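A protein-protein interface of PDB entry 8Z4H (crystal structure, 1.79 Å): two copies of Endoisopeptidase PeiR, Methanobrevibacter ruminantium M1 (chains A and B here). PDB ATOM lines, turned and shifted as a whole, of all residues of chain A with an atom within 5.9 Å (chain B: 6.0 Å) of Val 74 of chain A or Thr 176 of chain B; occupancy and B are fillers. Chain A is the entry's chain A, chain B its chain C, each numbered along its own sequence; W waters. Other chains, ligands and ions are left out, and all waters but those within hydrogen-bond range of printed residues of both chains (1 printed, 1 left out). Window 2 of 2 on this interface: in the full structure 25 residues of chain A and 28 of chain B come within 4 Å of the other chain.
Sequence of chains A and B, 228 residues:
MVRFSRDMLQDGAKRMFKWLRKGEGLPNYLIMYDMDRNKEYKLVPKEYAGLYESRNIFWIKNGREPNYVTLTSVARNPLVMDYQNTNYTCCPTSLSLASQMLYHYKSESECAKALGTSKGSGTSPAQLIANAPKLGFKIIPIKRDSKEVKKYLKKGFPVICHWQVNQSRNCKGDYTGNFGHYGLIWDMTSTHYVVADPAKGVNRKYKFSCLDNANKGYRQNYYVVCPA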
ATOM      1  N   MET A   1      -3.451 -16.862  26.818  1.00  0.00           N
ATOM      2  CA  MET A   1      -3.617 -16.825  25.341  1.00  0.00           C
ATOM      3  C   MET A   1      -2.697 -15.739  24.763  1.00  0.00           C
ATOM      4  O   MET A   1      -2.102 -14.994  25.541  1.00  0.00           O
ATOM      5  CB  MET A   1      -5.082 -16.576  24.970  1.00  0.00           C
ATOM      6  CG  MET A   1      -6.037 -17.641  25.489  1.00  0.00           C
ATOM      7  SD  MET A   1      -7.772 -17.141  25.666  1.00  0.00           S
ATOM      8  CE  MET A   1      -8.008 -17.332  27.427  1.00  0.00           C
ATOM      9  N   LYS A  46      -9.855 -14.562   9.901  1.00  0.00           N
ATOM     10  CA  LYS A  46     -10.774 -14.806  11.034  1.00  0.00           C
ATOM     11  C   LYS A  46     -10.123 -14.363  12.346  1.00  0.00           C
ATOM     12  O   LYS A  46     -10.871 -13.967  13.236  1.00  0.00           O
ATOM     13  CB  LYS A  46     -11.180 -16.278  11.090  1.00  0.00           C
ATOM     14  CG  LYS A  46     -12.178 -16.691  10.022  1.00  0.00           C
ATOM     15  CD  LYS A  46     -12.330 -18.187   9.874  1.00  0.00           C
ATOM     16  CE  LYS A  46     -11.540 -19.012  10.867  1.00  0.00           C
ATOM     17  NZ  LYS A  46     -11.453 -20.425  10.432  1.00  0.00           N
ATOM     18  N   GLU A  47      -8.789 -14.434  12.448  1.00  0.00           N
ATOM     19  CA  GLU A  47      -8.109 -14.054  13.709  1.00  0.00           C
ATOM     20  C   GLU A  47      -7.937 -12.538  13.786  1.00  0.00           C
ATOM     21  O   GLU A  47      -8.158 -11.974  14.850  1.00  0.00           O
ATOM     22  CB  GLU A  47      -6.725 -14.685  13.780  1.00  0.00           C
ATOM     23  CG  GLU A  47      -6.771 -16.161  14.067  1.00  0.00           C
ATOM     24  CD  GLU A  47      -5.446 -16.887  14.011  1.00  0.00           C
ATOM     25  OE1 GLU A  47      -4.714 -16.670  13.056  1.00  0.00           O
ATOM     26  OE2 GLU A  47      -5.193 -17.682  14.906  1.00  0.00           O
ATOM     27  N   ALA A  49      -9.770 -10.368  12.198  1.00  0.00           N
ATOM     28  CA  ALA A  49     -11.105  -9.796  12.368  1.00  0.00           C
ATOM     29  C   ALA A  49     -11.602  -9.943  13.813  1.00  0.00           C
ATOM     30  O   ALA A  49     -12.214  -9.021  14.354  1.00  0.00           O
ATOM     31  CB  ALA A  49     -12.093 -10.423  11.385  1.00  0.00           C
ATOM     32  N   GLY A  50     -11.339 -11.086  14.454  1.00  0.00           N
ATOM     33  CA  GLY A  50     -11.781 -11.280  15.825  1.00  0.00           C
ATOM     34  C   GLY A  50     -11.024 -10.416  16.811  1.00  0.00           C
ATOM     35  O   GLY A  50     -11.591  -9.875  17.759  1.00  0.00           O
ATOM     36  N   GLU A  53     -12.334  -6.910  16.347  1.00  0.00           N
ATOM     37  CA  GLU A  53     -13.675  -6.875  16.924  1.00  0.00           C
ATOM     38  C   GLU A  53     -13.605  -6.632  18.422  1.00  0.00           C
ATOM     39  O   GLU A  53     -14.315  -5.759  18.948  1.00  0.00           O
ATOM     40  CB  GLU A  53     -14.425  -8.177  16.619  1.00  0.00           C
ATOM     41  CG  GLU A  53     -15.882  -8.223  17.165  1.00  0.00           C
ATOM     42  CD  GLU A  53     -16.540  -9.585  16.931  1.00  0.00           C
ATOM     43  OE1 GLU A  53     -16.049 -10.617  17.408  1.00  0.00           O
ATOM     44  OE2 GLU A  53     -17.547  -9.637  16.204  1.00  0.00           O
ATOM     45  N   LEU A  71      -6.166 -12.410  22.084  1.00  0.00           N
ATOM     46  CA  LEU A  71      -6.823 -13.104  20.977  1.00  0.00           C
ATOM     47  C   LEU A  71      -7.628 -14.276  21.521  1.00  0.00           C
ATOM     48  O   LEU A  71      -7.062 -15.310  21.924  1.00  0.00           O
ATOM     49  CB  LEU A  71      -5.786 -13.545  19.947  1.00  0.00           C
ATOM     50  CG  LEU A  71      -6.273 -14.362  18.759  1.00  0.00           C
ATOM     51  CD1 LEU A  71      -6.823 -13.459  17.685  1.00  0.00           C
ATOM     52  CD2 LEU A  71      -5.116 -15.171  18.232  1.00  0.00           C
ATOM     53  N   THR A  72      -8.953 -14.136  21.503  1.00  0.00           N
ATOM     54  CA  THR A  72      -9.853 -15.116  22.106  1.00  0.00           C
ATOM     55  C   THR A  72     -10.883 -15.690  21.133  1.00  0.00           C
ATOM     56  O   THR A  72     -11.531 -16.698  21.453  1.00  0.00           O
ATOM     57  CB  THR A  72     -10.600 -14.477  23.298  1.00  0.00           C
ATOM     58  OG1 THR A  72     -11.338 -13.332  22.848  1.00  0.00           O
ATOM     59  CG2 THR A  72      -9.609 -14.019  24.359  1.00  0.00           C
ATOM     60  N   SER A  73     -11.049 -15.090  19.961  1.00  0.00           N
ATOM     61  CA  SER A  73     -12.236 -15.312  19.147  1.00  0.00           C
ATOM     62  C   SER A  73     -11.874 -15.113  17.677  1.00  0.00           C
ATOM     63  O   SER A  73     -10.801 -14.602  17.344  1.00  0.00           O
ATOM     64  CB  SER A  73     -13.364 -14.368  19.581  1.00  0.00           C
ATOM     65  OG  SER A  73     -12.934 -13.011  19.468  1.00  0.00           O
ATOM     66  N   VAL A  74     -12.823 -15.505  16.850  1.00  0.00           N
ATOM     67  CA  VAL A  74     -12.756 -15.309  15.388  1.00  0.00           C
ATOM     68  C   VAL A  74     -14.037 -14.586  14.960  1.00  0.00           C
ATOM     69  O   VAL A  74     -14.999 -14.599  15.696  1.00  0.00           O
ATOM     70  CB  VAL A  74     -12.565 -16.641  14.659  1.00  0.00           C
ATOM     71  CG1 VAL A  74     -11.265 -17.309  15.080  1.00  0.00           C
ATOM     72  CG2 VAL A  74     -13.744 -17.553  14.889  1.00  0.00           C
ATOM     73  N   ALA A  75     -13.999 -13.946  13.806  1.00  0.00           N
ATOM     74  CA  ALA A  75     -15.154 -13.209  13.260  1.00  0.00           C
ATOM     75  C   ALA A  75     -14.921 -13.017  11.761  1.00  0.00           C
ATOM     76  O   ALA A  75     -13.792 -13.016  11.362  1.00  0.00           O
ATOM     77  CB  ALA A  75     -15.314 -11.903  13.979  1.00  0.00           C
ATOM     78  N   ARG A  76     -15.984 -12.837  11.009  1.00  0.00           N
ATOM     79  CA  ARG A  76     -15.776 -12.655   9.564  1.00  0.00           C
ATOM     80  C   ARG A  76     -15.430 -11.190   9.291  1.00  0.00           C
ATOM     81  O   ARG A  76     -15.017 -10.910   8.198  1.00  0.00           O
ATOM     82  CB  ARG A  76     -16.899 -13.316   8.765  1.00  0.00           C
ATOM     83  CG  ARG A  76     -16.395 -14.378   7.787  1.00  0.00           C
ATOM     84  CD  ARG A  76     -15.351 -15.425   8.213  1.00  0.00           C
ATOM     85  NE  ARG A  76     -13.944 -15.225   7.849  1.00  0.00           N
ATOM     86  CZ  ARG A  76     -13.244 -16.017   7.035  1.00  0.00           C
ATOM     87  NH1 ARG A  76     -13.817 -17.070   6.470  1.00  0.00           N
ATOM     88  NH2 ARG A  76     -11.969 -15.764   6.786  1.00  0.00           N
ATOM     89  N   VAL B 165     -16.364 -21.767  26.771  1.00  0.00           N
ATOM     90  CA  VAL B 165     -16.287 -21.495  25.299  1.00  0.00           C
ATOM     91  C   VAL B 165     -15.440 -22.531  24.581  1.00  0.00           C
ATOM     92  O   VAL B 165     -15.722 -22.788  23.428  1.00  0.00           O
ATOM     93  CB  VAL B 165     -15.862 -20.061  24.948  1.00  0.00           C
ATOM     94  CG1 VAL B 165     -16.746 -19.043  25.627  1.00  0.00           C
ATOM     95  CG2 VAL B 165     -14.408 -19.821  25.264  1.00  0.00           C
ATOM     96  N   ARG B 169     -16.116 -24.930  20.729  1.00  0.00           N
ATOM     97  CA  ARG B 169     -15.221 -24.657  19.596  1.00  0.00           C
ATOM     98  C   ARG B 169     -15.642 -25.387  18.319  1.00  0.00           C
ATOM     99  O   ARG B 169     -15.720 -24.773  17.249  1.00  0.00           O
ATOM    100  CB  ARG B 169     -13.781 -25.001  19.961  1.00  0.00           C
ATOM    101  CG  ARG B 169     -12.903 -25.296  18.754  1.00  0.00           C
ATOM    102  CD  ARG B 169     -11.910 -24.199  18.413  1.00  0.00           C
ATOM    103  NE  ARG B 169     -11.177 -24.580  17.208  1.00  0.00           N
ATOM    104  CZ  ARG B 169     -10.085 -23.981  16.748  1.00  0.00           C
ATOM    105  NH1 ARG B 169      -9.518 -22.978  17.401  1.00  0.00           N
ATOM    106  NH2 ARG B 169      -9.534 -24.417  15.614  1.00  0.00           N
ATOM    107  N   GLY B 173     -17.837 -22.535  17.143  1.00  0.00           N
ATOM    108  CA  GLY B 173     -16.689 -21.904  16.515  1.00  0.00           C
ATOM    109  C   GLY B 173     -16.520 -20.405  16.686  1.00  0.00           C
ATOM    110  O   GLY B 173     -16.041 -19.738  15.756  1.00  0.00           O
ATOM    111  N   ASP B 174     -16.998 -19.832  17.786  1.00  0.00           N
ATOM    112  CA  ASP B 174     -16.885 -18.392  18.028  1.00  0.00           C
ATOM    113  C   ASP B 174     -15.586 -18.037  18.742  1.00  0.00           C
ATOM    114  O   ASP B 174     -15.121 -16.898  18.644  1.00  0.00           O
ATOM    115  CB  ASP B 174     -18.084 -17.889  18.859  1.00  0.00           C
ATOM    116  CG  ASP B 174     -19.183 -17.270  18.017  1.00  0.00           C
ATOM    117  OD1 ASP B 174     -19.215 -17.505  16.792  1.00  0.00           O
ATOM    118  OD2 ASP B 174     -20.084 -16.579  18.599  1.00  0.00           O
ATOM    119  N   TYR B 175     -15.048 -18.961  19.536  1.00  0.00           N
ATOM    120  CA  TYR B 175     -13.958 -18.686  20.465  1.00  0.00           C
ATOM    121  C   TYR B 175     -12.812 -19.668  20.252  1.00  0.00           C
ATOM    122  O   TYR B 175     -13.030 -20.798  19.808  1.00  0.00           O
ATOM    123  CB  TYR B 175     -14.424 -18.760  21.926  1.00  0.00           C
ATOM    124  CG  TYR B 175     -15.442 -17.702  22.286  1.00  0.00           C
ATOM    125  CD1 TYR B 175     -15.027 -16.424  22.691  1.00  0.00           C
ATOM    126  CD2 TYR B 175     -16.813 -17.970  22.210  1.00  0.00           C
ATOM    127  CE1 TYR B 175     -15.957 -15.422  23.002  1.00  0.00           C
ATOM    128  CE2 TYR B 175     -17.760 -16.980  22.525  1.00  0.00           C
ATOM    129  CZ  TYR B 175     -17.323 -15.712  22.916  1.00  0.00           C
ATOM    130  OH  TYR B 175     -18.238 -14.737  23.260  1.00  0.00           O
ATOM    131  N   THR B 176     -11.603 -19.252  20.607  1.00  0.00           N
ATOM    132  CA  THR B 176     -10.419 -20.134  20.517  1.00  0.00           C
ATOM    133  C   THR B 176      -9.764 -20.224  21.896  1.00  0.00           C
ATOM    134  O   THR B 176      -8.858 -21.021  22.052  1.00  0.00           O
ATOM    135  CB  THR B 176      -9.415 -19.667  19.454  1.00  0.00           C
ATOM    136  OG1 THR B 176      -8.837 -18.424  19.831  1.00  0.00           O
ATOM    137  CG2 THR B 176      -9.991 -19.562  18.068  1.00  0.00           C
ATOM    138  N   GLY B 177     -10.225 -19.423  22.846  1.00  0.00           N
ATOM    139  CA  GLY B 177      -9.645 -19.396  24.198  1.00  0.00           C
ATOM    140  C   GLY B 177     -10.269 -20.406  25.143  1.00  0.00           C
ATOM    141  O   GLY B 177     -11.083 -21.206  24.688  1.00  0.00           O
ATOM    142  N   ASN B 178      -9.887 -20.319  26.414  1.00  0.00           N
ATOM    143  CA  ASN B 178     -10.393 -21.221  27.469  1.00  0.00           C
ATOM    144  C   ASN B 178     -10.824 -20.404  28.680  1.00  0.00           C
ATOM    145  O   ASN B 178      -9.965 -19.910  29.410  1.00  0.00           O
ATOM    146  CB  ASN B 178      -9.370 -22.268  27.886  1.00  0.00           C
ATOM    147  CG  ASN B 178      -9.482 -23.519  27.055  1.00  0.00           C
ATOM    148  OD1 ASN B 178     -10.529 -23.796  26.482  1.00  0.00           O
ATOM    149  ND2 ASN B 178      -8.397 -24.261  26.961  1.00  0.00           N
ATOM    150  N   LYS B 200     -19.724 -10.978  21.675  1.00  0.00           N
ATOM    151  CA  LYS B 200     -19.797 -11.370  20.268  1.00  0.00           C
ATOM    152  C   LYS B 200     -20.951 -10.718  19.491  1.00  0.00           C
ATOM    153  O   LYS B 200     -20.716 -10.193  18.392  1.00  0.00           O
ATOM    154  CB  LYS B 200     -19.902 -12.888  20.133  1.00  0.00           C
ATOM    155  CG  LYS B 200     -18.532 -13.658  20.245  1.00  0.00           C
ATOM    156  CD  LYS B 200     -17.479 -13.164  19.220  1.00  0.00           C
ATOM    157  CE  LYS B 200     -17.794 -13.655  17.825  1.00  0.00           C
ATOM    158  NZ  LYS B 200     -17.217 -12.798  16.747  1.00  0.00           N
ATOM    159  N   ARG B 204     -26.294 -14.912  18.370  1.00  0.00           N
ATOM    160  CA  ARG B 204     -25.375 -16.049  18.183  1.00  0.00           C
ATOM    161  C   ARG B 204     -26.165 -17.342  18.365  1.00  0.00           C
ATOM    162  O   ARG B 204     -26.708 -17.598  19.442  1.00  0.00           O
ATOM    163  CB  ARG B 204     -24.185 -15.971  19.131  1.00  0.00           C
ATOM    164  CG  ARG B 204     -23.640 -14.582  19.331  1.00  0.00           C
ATOM    165  CD  ARG B 204     -23.115 -13.987  18.051  1.00  0.00           C
ATOM    166  NE  ARG B 204     -22.140 -14.863  17.414  1.00  0.00           N
ATOM    167  CZ  ARG B 204     -21.688 -14.692  16.180  1.00  0.00           C
ATOM    168  NH1 ARG B 204     -22.132 -13.700  15.419  1.00  0.00           N
ATOM    169  NH2 ARG B 204     -20.754 -15.521  15.710  1.00  0.00           N
HETATM  170  O   HOH W   1     -19.215  -7.268  17.409  1.00  0.00           O
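Of the printed residues of chain B, Val 74 of chain A touches Gly 173, Asp 174, Thr 176 and Lys 200.
Of the printed residues of chain A, Thr 176 of chain B touches Thr 72 and Val 74.
Of the printed residues of chain A, Gly 173 of chain B touches Val 74.
Of the printed residues of chain A, Asn 178 of chain B touches Met 1 (3.7 Å).
Of the printed residues of chain B, Met 1 of chain A touches Gly 177 and Asn 178.
Of the printed residues of chain A, Lys 200 of chain B touches Glu 53, Val 74 and Ala 75.
Of the printed residues of chain A, Gly 177 of chain B touches Met 1 (3.3 Å) and Thr 72 (3.3 Å).
The nearest printed residue of chain A that does not touch Thr 176 of chain B is Ser 73 of chain A (4.003 Å).
Water W1 lies within hydrogen-bond range of OE2 of Glu 53 of chain A (3.1 Å) and O of Lys 200 of chain B (3.4 Å).
The backbone carbonyl oxygen (O) of Thr 72 of chain A lies within hydrogen-bond range of the backbone NH (N) of Thr 176 of chain B, at 2.7 Å.
O of Asp 174 of chain B lies within hydrogen-bond range of N of Val 74 of chain A (3.2 Å).
The backbone NH of Gly 177 of chain B sits at hydrogen-bond distance from the backbone carbonyl oxygen of Thr 72 of chain A (3.3 Å).
The side-chain carboxylate (OE1) of Glu 53 of chain A lies within salt-bridge range of the side-chain amino group (NZ) of Lys 200 of chain B (2.6 Å).
NZ of Lys 200 of chain B sits at hydrogen-bond distance from O of Val 74 of chain A.
Among the printed residues, merely in contact across the chains: Met 1 of chain A with Gly 177 of chain B (3.3 Å), Met 1 of chain A with Asn 178 of chain B (3.7 Å), Thr 72 of chain A with Tyr 175 of chain B (3.3 Å), Ser 73 of chain A with Asp 174 of chain B (3.2 Å), Val 74 of chain A with Gly 173 of chain B (3.3 Å), Val 74 of chain A with Thr 176 of chain B (3.95 Å) and Ala 75 of chain A with Lys 200 of chain B (3.5 Å).
Of the 10 printed residues of chain B, 7 touch a printed residue of chain A.
Printed residues of chain B that touch a printed residue of chain A: Gly 173, Asp 174, Tyr 175, Thr 176, Gly 177, Asn 178 and Lys 200.
Hydrophobic or aromatic side chains of chain B that line the printed part of chain A: Tyr 175.
Among the printed residues, 12 pairs touch across the chains.
No position is printed for both chains.
Of the 12 pairs that touch across the chains among the printed residues, none has its exchanged pair printed and touching as well.
NH2 of Arg 204 of chain B is in salt-bridge range of OD1 of Asp 174 of chain B, at 2.7 Å.
The backbone carbonyl oxygen (O) of Lys 46 of chain A is in hydrogen-bond range of the backbone NH (N) of Ala 75 of chain A, 3.2 Å away.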
